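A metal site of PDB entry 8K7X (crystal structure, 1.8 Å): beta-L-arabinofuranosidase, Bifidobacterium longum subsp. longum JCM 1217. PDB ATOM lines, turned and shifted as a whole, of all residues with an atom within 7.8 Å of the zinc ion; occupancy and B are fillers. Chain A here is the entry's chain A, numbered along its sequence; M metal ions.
The side-chain carboxylate (OE1) of Glu 345 lies close to the side-chain amide oxygen (OD1) of Asn 348 (3.4 Å). SG of Cys 427 sits close to N of Thr 346, at 3.6 Å. The side-chain hydroxyl (OG1) of Thr 430 is in hydrogen-bond range of the backbone carbonyl oxygen (O) of Cys 427, at 3.4 Å. The side-chain hydroxyl (OG1) of Thr 430 sits close to the side-chain sulfur (SG) of Cys 347 (3.3 Å). The side-chain sulfur (SG) of Cys 426 sits close to the side-chain hydroxyl (OH) of Tyr 393 (3.4 Å). The backbone carbonyl oxygen of Cys 426 sits at hydrogen-bond distance from the side-chain hydroxyl of Thr 430 (3.4 Å).
The zinc ion is bound by OE2 of Glu 345 (2.0 Å), SG of Cys 427 (2.3 Å), SG of Cys 347 (2.3 Å) and SG of Cys 426 (2.4 Å).
Of the 23 residues printed, 4 come within 4 Å of the zinc ion. The nearest printed residue that does not touch the zinc ion is Tyr 393 (4.1 Å).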
ATOM      1  N   TRP A  51     -27.240  -6.421  25.470  1.00  0.00           N
ATOM      2  CA  TRP A  51     -26.676  -5.877  26.700  1.00  0.00           C
ATOM      3  C   TRP A  51     -27.727  -5.806  27.809  1.00  0.00           C
ATOM      4  O   TRP A  51     -27.335  -5.563  28.940  1.00  0.00           O
ATOM      5  CB  TRP A  51     -26.045  -4.491  26.506  1.00  0.00           C
ATOM      6  CG  TRP A  51     -24.833  -4.475  25.637  1.00  0.00           C
ATOM      7  CD1 TRP A  51     -24.454  -5.357  24.679  1.00  0.00           C
ATOM      8  CD2 TRP A  51     -23.785  -3.493  25.681  1.00  0.00           C
ATOM      9  NE1 TRP A  51     -23.282  -4.961  24.069  1.00  0.00           N
ATOM     10  CE2 TRP A  51     -22.867  -3.815  24.673  1.00  0.00           C
ATOM     11  CE3 TRP A  51     -23.557  -2.365  26.464  1.00  0.00           C
ATOM     12  CZ2 TRP A  51     -21.706  -3.085  24.464  1.00  0.00           C
ATOM     13  CZ3 TRP A  51     -22.411  -1.630  26.236  1.00  0.00           C
ATOM     14  CH2 TRP A  51     -21.518  -1.997  25.255  1.00  0.00           C
ATOM     15  N   HIS A  73     -28.635  -0.447  31.788  1.00  0.00           N
ATOM     16  CA  HIS A  73     -27.975   0.729  31.231  1.00  0.00           C
ATOM     17  C   HIS A  73     -28.876   1.383  30.165  1.00  0.00           C
ATOM     18  O   HIS A  73     -29.064   2.617  30.154  1.00  0.00           O
ATOM     19  CB  HIS A  73     -26.545   0.463  30.683  1.00  0.00           C
ATOM     20  CG  HIS A  73     -26.531   0.001  29.284  1.00  0.00           C
ATOM     21  ND1 HIS A  73     -26.330   0.930  28.272  1.00  0.00           N
ATOM     22  CD2 HIS A  73     -26.834  -1.179  28.687  1.00  0.00           C
ATOM     23  CE1 HIS A  73     -26.476   0.307  27.093  1.00  0.00           C
ATOM     24  NE2 HIS A  73     -26.775  -0.994  27.314  1.00  0.00           N
ATOM     25  N   HIS A  77     -31.142   4.938  29.840  1.00  0.00           N
ATOM     26  CA  HIS A  77     -31.089   5.860  28.702  1.00  0.00           C
ATOM     27  C   HIS A  77     -32.490   6.094  28.138  1.00  0.00           C
ATOM     28  O   HIS A  77     -32.833   7.211  27.715  1.00  0.00           O
ATOM     29  CB  HIS A  77     -30.160   5.359  27.590  1.00  0.00           C
ATOM     30  CG  HIS A  77     -28.728   5.480  27.911  1.00  0.00           C
ATOM     31  ND1 HIS A  77     -28.120   6.708  28.003  1.00  0.00           N
ATOM     32  CD2 HIS A  77     -27.733   4.550  28.029  1.00  0.00           C
ATOM     33  CE1 HIS A  77     -26.829   6.530  28.229  1.00  0.00           C
ATOM     34  NE2 HIS A  77     -26.550   5.235  28.185  1.00  0.00           N
ATOM     35  N   TYR A 148     -21.850   1.905  36.444  1.00  0.00           N
ATOM     36  CA  TYR A 148     -22.111   2.528  35.161  1.00  0.00           C
ATOM     37  C   TYR A 148     -23.578   2.316  34.765  1.00  0.00           C
ATOM     38  O   TYR A 148     -24.277   3.228  34.298  1.00  0.00           O
ATOM     39  CB  TYR A 148     -21.141   2.001  34.100  1.00  0.00           C
ATOM     40  CG  TYR A 148     -21.440   2.404  32.682  1.00  0.00           C
ATOM     41  CD1 TYR A 148     -22.433   1.764  31.951  1.00  0.00           C
ATOM     42  CD2 TYR A 148     -20.787   3.479  32.089  1.00  0.00           C
ATOM     43  CE1 TYR A 148     -22.719   2.123  30.646  1.00  0.00           C
ATOM     44  CE2 TYR A 148     -21.005   3.794  30.760  1.00  0.00           C
ATOM     45  CZ  TYR A 148     -22.023   3.171  30.062  1.00  0.00           C
ATOM     46  OH  TYR A 148     -22.333   3.557  28.787  1.00  0.00           O
ATOM     47  N   HIS A 250      -9.339   4.760  29.735  1.00  0.00           N
ATOM     48  CA  HIS A 250     -10.541   4.566  28.934  1.00  0.00           C
ATOM     49  C   HIS A 250     -11.243   5.921  28.806  1.00  0.00           C
ATOM     50  O   HIS A 250     -11.520   6.564  29.814  1.00  0.00           O
ATOM     51  CB  HIS A 250     -11.394   3.479  29.601  1.00  0.00           C
ATOM     52  CG  HIS A 250     -12.558   3.099  28.787  1.00  0.00           C
ATOM     53  ND1 HIS A 250     -13.747   3.825  28.718  1.00  0.00           N
ATOM     54  CD2 HIS A 250     -12.673   2.067  27.957  1.00  0.00           C
ATOM     55  CE1 HIS A 250     -14.524   3.202  27.845  1.00  0.00           C
ATOM     56  NE2 HIS A 250     -13.912   2.142  27.380  1.00  0.00           N
ATOM     57  N   ASN A 252     -14.327   7.130  27.348  1.00  0.00           N
ATOM     58  CA  ASN A 252     -15.696   7.343  27.791  1.00  0.00           C
ATOM     59  C   ASN A 252     -15.890   7.133  29.302  1.00  0.00           C
ATOM     60  O   ASN A 252     -16.829   7.686  29.910  1.00  0.00           O
ATOM     61  CB  ASN A 252     -16.688   6.497  27.018  1.00  0.00           C
ATOM     62  CG  ASN A 252     -18.100   7.016  27.204  1.00  0.00           C
ATOM     63  OD1 ASN A 252     -18.391   8.185  26.988  1.00  0.00           O
ATOM     64  ND2 ASN A 252     -18.997   6.152  27.656  1.00  0.00           N
ATOM     65  N   GLU A 316     -11.400   2.483  22.308  1.00  0.00           N
ATOM     66  CA  GLU A 316     -12.076   3.078  23.461  1.00  0.00           C
ATOM     67  C   GLU A 316     -11.160   3.790  24.462  1.00  0.00           C
ATOM     68  O   GLU A 316     -11.650   4.219  25.525  1.00  0.00           O
ATOM     69  CB  GLU A 316     -12.935   2.059  24.197  1.00  0.00           C
ATOM     70  CG  GLU A 316     -14.047   1.453  23.335  1.00  0.00           C
ATOM     71  CD  GLU A 316     -15.067   0.593  24.084  1.00  0.00           C
ATOM     72  OE1 GLU A 316     -15.210   0.787  25.294  1.00  0.00           O
ATOM     73  OE2 GLU A 316     -15.808  -0.178  23.441  1.00  0.00           O
ATOM     74  N   GLU A 345     -15.409   6.131  19.379  1.00  0.00           N
ATOM     75  CA  GLU A 345     -16.614   5.679  20.020  1.00  0.00           C
ATOM     76  C   GLU A 345     -17.560   6.876  20.098  1.00  0.00           C
ATOM     77  O   GLU A 345     -17.102   7.955  20.458  1.00  0.00           O
ATOM     78  CB  GLU A 345     -16.313   5.092  21.401  1.00  0.00           C
ATOM     79  CG  GLU A 345     -17.578   4.664  22.154  1.00  0.00           C
ATOM     80  CD  GLU A 345     -17.466   4.103  23.555  1.00  0.00           C
ATOM     81  OE1 GLU A 345     -16.326   3.909  24.046  1.00  0.00           O
ATOM     82  OE2 GLU A 345     -18.555   3.857  24.174  1.00  0.00           O
ATOM     83  N   THR A 346     -18.846   6.695  19.794  1.00  0.00           N
ATOM     84  CA  THR A 346     -19.802   7.802  19.718  1.00  0.00           C
ATOM     85  C   THR A 346     -20.250   8.308  21.089  1.00  0.00           C
ATOM     86  O   THR A 346     -20.506   9.517  21.245  1.00  0.00           O
ATOM     87  CB  THR A 346     -20.917   7.427  18.745  1.00  0.00           C
ATOM     88  OG1 THR A 346     -20.344   7.028  17.490  1.00  0.00           O
ATOM     89  CG2 THR A 346     -21.882   8.568  18.473  1.00  0.00           C
ATOM     90  N   CYS A 347     -20.397   7.446  22.114  1.00  0.00           N
ATOM     91  CA  CYS A 347     -20.683   7.896  23.477  1.00  0.00           C
ATOM     92  C   CYS A 347     -19.780   9.088  23.866  1.00  0.00           C
ATOM     93  O   CYS A 347     -20.216  10.024  24.548  1.00  0.00           O
ATOM     94  CB  CYS A 347     -20.397   6.837  24.528  1.00  0.00           C
ATOM     95  SG  CYS A 347     -21.660   5.537  24.576  1.00  0.00           S
ATOM     96  N   ASN A 348     -18.525   9.003  23.466  1.00  0.00           N
ATOM     97  CA  ASN A 348     -17.522   9.962  23.893  1.00  0.00           C
ATOM     98  C   ASN A 348     -17.930  11.371  23.503  1.00  0.00           C
ATOM     99  O   ASN A 348     -17.665  12.301  24.266  1.00  0.00           O
ATOM    100  CB  ASN A 348     -16.138   9.676  23.317  1.00  0.00           C
ATOM    101  CG  ASN A 348     -15.646   8.260  23.618  1.00  0.00           C
ATOM    102  OD1 ASN A 348     -16.423   7.327  23.801  1.00  0.00           O
ATOM    103  ND2 ASN A 348     -14.349   8.078  23.570  1.00  0.00           N
ATOM    104  N   ASN A 351     -20.775  12.752  25.590  1.00  0.00           N
ATOM    105  CA  ASN A 351     -20.196  13.239  26.842  1.00  0.00           C
ATOM    106  C   ASN A 351     -19.393  14.529  26.637  1.00  0.00           C
ATOM    107  O   ASN A 351     -19.488  15.410  27.485  1.00  0.00           O
ATOM    108  CB  ASN A 351     -19.459  12.099  27.549  1.00  0.00           C
ATOM    109  CG  ASN A 351     -20.419  11.232  28.340  1.00  0.00           C
ATOM    110  OD1 ASN A 351     -21.247  11.743  29.093  1.00  0.00           O
ATOM    111  ND2 ASN A 351     -20.402   9.940  28.107  1.00  0.00           N
ATOM    112  N   THR A 392     -24.310   4.854  15.268  1.00  0.00           N
ATOM    113  CA  THR A 392     -22.992   4.240  15.220  1.00  0.00           C
ATOM    114  C   THR A 392     -22.421   3.920  16.625  1.00  0.00           C
ATOM    115  O   THR A 392     -22.770   4.548  17.630  1.00  0.00           O
ATOM    116  CB  THR A 392     -22.007   5.168  14.502  1.00  0.00           C
ATOM    117  OG1 THR A 392     -21.989   6.430  15.157  1.00  0.00           O
ATOM    118  CG2 THR A 392     -22.350   5.367  13.060  1.00  0.00           C
ATOM    119  N   TYR A 393     -21.514   2.934  16.660  1.00  0.00           N
ATOM    120  CA  TYR A 393     -20.588   2.700  17.751  1.00  0.00           C
ATOM    121  C   TYR A 393     -19.306   3.474  17.443  1.00  0.00           C
ATOM    122  O   TYR A 393     -19.193   4.669  17.759  1.00  0.00           O
ATOM    123  CB  TYR A 393     -20.414   1.203  18.042  1.00  0.00           C
ATOM    124  CG  TYR A 393     -19.879   0.927  19.422  1.00  0.00           C
ATOM    125  CD1 TYR A 393     -18.576   1.209  19.760  1.00  0.00           C
ATOM    126  CD2 TYR A 393     -20.671   0.339  20.393  1.00  0.00           C
ATOM    127  CE1 TYR A 393     -18.072   0.938  21.041  1.00  0.00           C
ATOM    128  CE2 TYR A 393     -20.197   0.055  21.673  1.00  0.00           C
ATOM    129  CZ  TYR A 393     -18.888   0.333  21.990  1.00  0.00           C
ATOM    130  OH  TYR A 393     -18.464   0.059  23.276  1.00  0.00           O
ATOM    131  N   PHE A 394     -18.384   2.856  16.698  1.00  0.00           N
ATOM    132  CA  PHE A 394     -17.200   3.551  16.252  1.00  0.00           C
ATOM    133  C   PHE A 394     -17.483   4.390  15.014  1.00  0.00           C
ATOM    134  O   PHE A 394     -18.449   4.140  14.274  1.00  0.00           O
ATOM    135  CB  PHE A 394     -16.085   2.549  16.007  1.00  0.00           C
ATOM    136  CG  PHE A 394     -15.685   1.761  17.218  1.00  0.00           C
ATOM    137  CD1 PHE A 394     -15.145   2.397  18.325  1.00  0.00           C
ATOM    138  CD2 PHE A 394     -15.812   0.388  17.234  1.00  0.00           C
ATOM    139  CE1 PHE A 394     -14.799   1.694  19.474  1.00  0.00           C
ATOM    140  CE2 PHE A 394     -15.459  -0.330  18.363  1.00  0.00           C
ATOM    141  CZ  PHE A 394     -14.960   0.325  19.474  1.00  0.00           C
ATOM    142  N   TRP A 425     -26.067  -1.443  22.597  1.00  0.00           N
ATOM    143  CA  TRP A 425     -24.782  -0.867  23.001  1.00  0.00           C
ATOM    144  C   TRP A 425     -24.968   0.412  23.808  1.00  0.00           C
ATOM    145  O   TRP A 425     -25.932   1.177  23.641  1.00  0.00           O
ATOM    146  CB  TRP A 425     -23.920  -0.523  21.772  1.00  0.00           C
ATOM    147  CG  TRP A 425     -23.913  -1.498  20.641  1.00  0.00           C
ATOM    148  CD1 TRP A 425     -23.782  -2.863  20.718  1.00  0.00           C
ATOM    149  CD2 TRP A 425     -23.910  -1.177  19.245  1.00  0.00           C
ATOM    150  NE1 TRP A 425     -23.838  -3.404  19.478  1.00  0.00           N
ATOM    151  CE2 TRP A 425     -23.875  -2.405  18.550  1.00  0.00           C
ATOM    152  CE3 TRP A 425     -23.968   0.004  18.517  1.00  0.00           C
ATOM    153  CZ2 TRP A 425     -23.850  -2.462  17.161  1.00  0.00           C
ATOM    154  CZ3 TRP A 425     -23.965  -0.066  17.125  1.00  0.00           C
ATOM    155  CH2 TRP A 425     -23.902  -1.294  16.467  1.00  0.00           C
ATOM    156  N   CYS A 426     -23.937   0.734  24.622  1.00  0.00           N
ATOM    157  CA  CYS A 426     -23.818   2.050  25.222  1.00  0.00           C
ATOM    158  C   CYS A 426     -24.094   3.131  24.174  1.00  0.00           C
ATOM    159  O   CYS A 426     -24.845   4.077  24.454  1.00  0.00           O
ATOM    160  CB  CYS A 426     -22.422   2.184  25.820  1.00  0.00           C
ATOM    161  SG  CYS A 426     -21.073   1.757  24.667  1.00  0.00           S
ATOM    162  N   CYS A 427     -23.477   3.009  22.987  1.00  0.00           N
ATOM    163  CA  CYS A 427     -23.556   4.010  21.951  1.00  0.00           C
ATOM    164  C   CYS A 427     -24.997   4.152  21.439  1.00  0.00           C
ATOM    165  O   CYS A 427     -25.374   5.198  20.946  1.00  0.00           O
ATOM    166  CB  CYS A 427     -22.551   3.745  20.816  1.00  0.00           C
ATOM    167  SG  CYS A 427     -20.813   4.093  21.291  1.00  0.00           S
ATOM    168  N   GLN A 428     -25.810   3.084  21.495  1.00  0.00           N
ATOM    169  CA  GLN A 428     -27.192   3.179  21.119  1.00  0.00           C
ATOM    170  C   GLN A 428     -27.989   3.901  22.180  1.00  0.00           C
ATOM    171  O   GLN A 428     -28.937   4.594  21.839  1.00  0.00           O
ATOM    172  CB  GLN A 428     -27.827   1.823  20.844  1.00  0.00           C
ATOM    173  CG  GLN A 428     -27.192   1.172  19.640  1.00  0.00           C
ATOM    174  CD  GLN A 428     -27.824  -0.162  19.327  1.00  0.00           C
ATOM    175  OE1 GLN A 428     -27.442  -1.213  19.842  1.00  0.00           O
ATOM    176  NE2 GLN A 428     -28.782  -0.110  18.425  1.00  0.00           N
ATOM    177  N   GLY A 429     -27.607   3.746  23.456  1.00  0.00           N
ATOM    178  CA  GLY A 429     -28.290   4.394  24.576  1.00  0.00           C
ATOM    179  C   GLY A 429     -27.980   5.903  24.657  1.00  0.00           C
ATOM    180  O   GLY A 429     -28.880   6.746  24.710  1.00  0.00           O
ATOM    181  N   THR A 430     -26.698   6.281  24.544  1.00  0.00           N
ATOM    182  CA  THR A 430     -26.426   7.699  24.341  1.00  0.00           C
ATOM    183  C   THR A 430     -27.056   8.208  23.047  1.00  0.00           C
ATOM    184  O   THR A 430     -27.500   9.354  22.983  1.00  0.00           O
ATOM    185  CB  THR A 430     -24.928   7.992  24.385  1.00  0.00           C
ATOM    186  OG1 THR A 430     -24.238   7.212  23.402  1.00  0.00           O
ATOM    187  CG2 THR A 430     -24.362   7.769  25.767  1.00  0.00           C
ATOM    188  N   GLY A 431     -27.072   7.356  22.004  1.00  0.00           N
ATOM    189  CA  GLY A 431     -27.698   7.686  20.733  1.00  0.00           C
ATOM    190  C   GLY A 431     -29.154   8.144  20.849  1.00  0.00           C
ATOM    191  O   GLY A 431     -29.565   9.120  20.244  1.00  0.00           O
ATOM    192  N   VAL A 584     -20.444  -6.004  19.891  1.00  0.00           N
ATOM    193  CA  VAL A 584     -20.313  -4.736  19.187  1.00  0.00           C
ATOM    194  C   VAL A 584     -20.021  -4.977  17.707  1.00  0.00           C
ATOM    195  O   VAL A 584     -19.049  -5.640  17.362  1.00  0.00           O
ATOM    196  CB  VAL A 584     -19.197  -3.887  19.819  1.00  0.00           C
ATOM    197  CG1 VAL A 584     -18.965  -2.597  19.015  1.00  0.00           C
ATOM    198  CG2 VAL A 584     -19.523  -3.537  21.289  1.00  0.00           C
HETATM  199 ZN    ZN M   1     -20.470   3.780  23.582  1.00  0.00          ZN
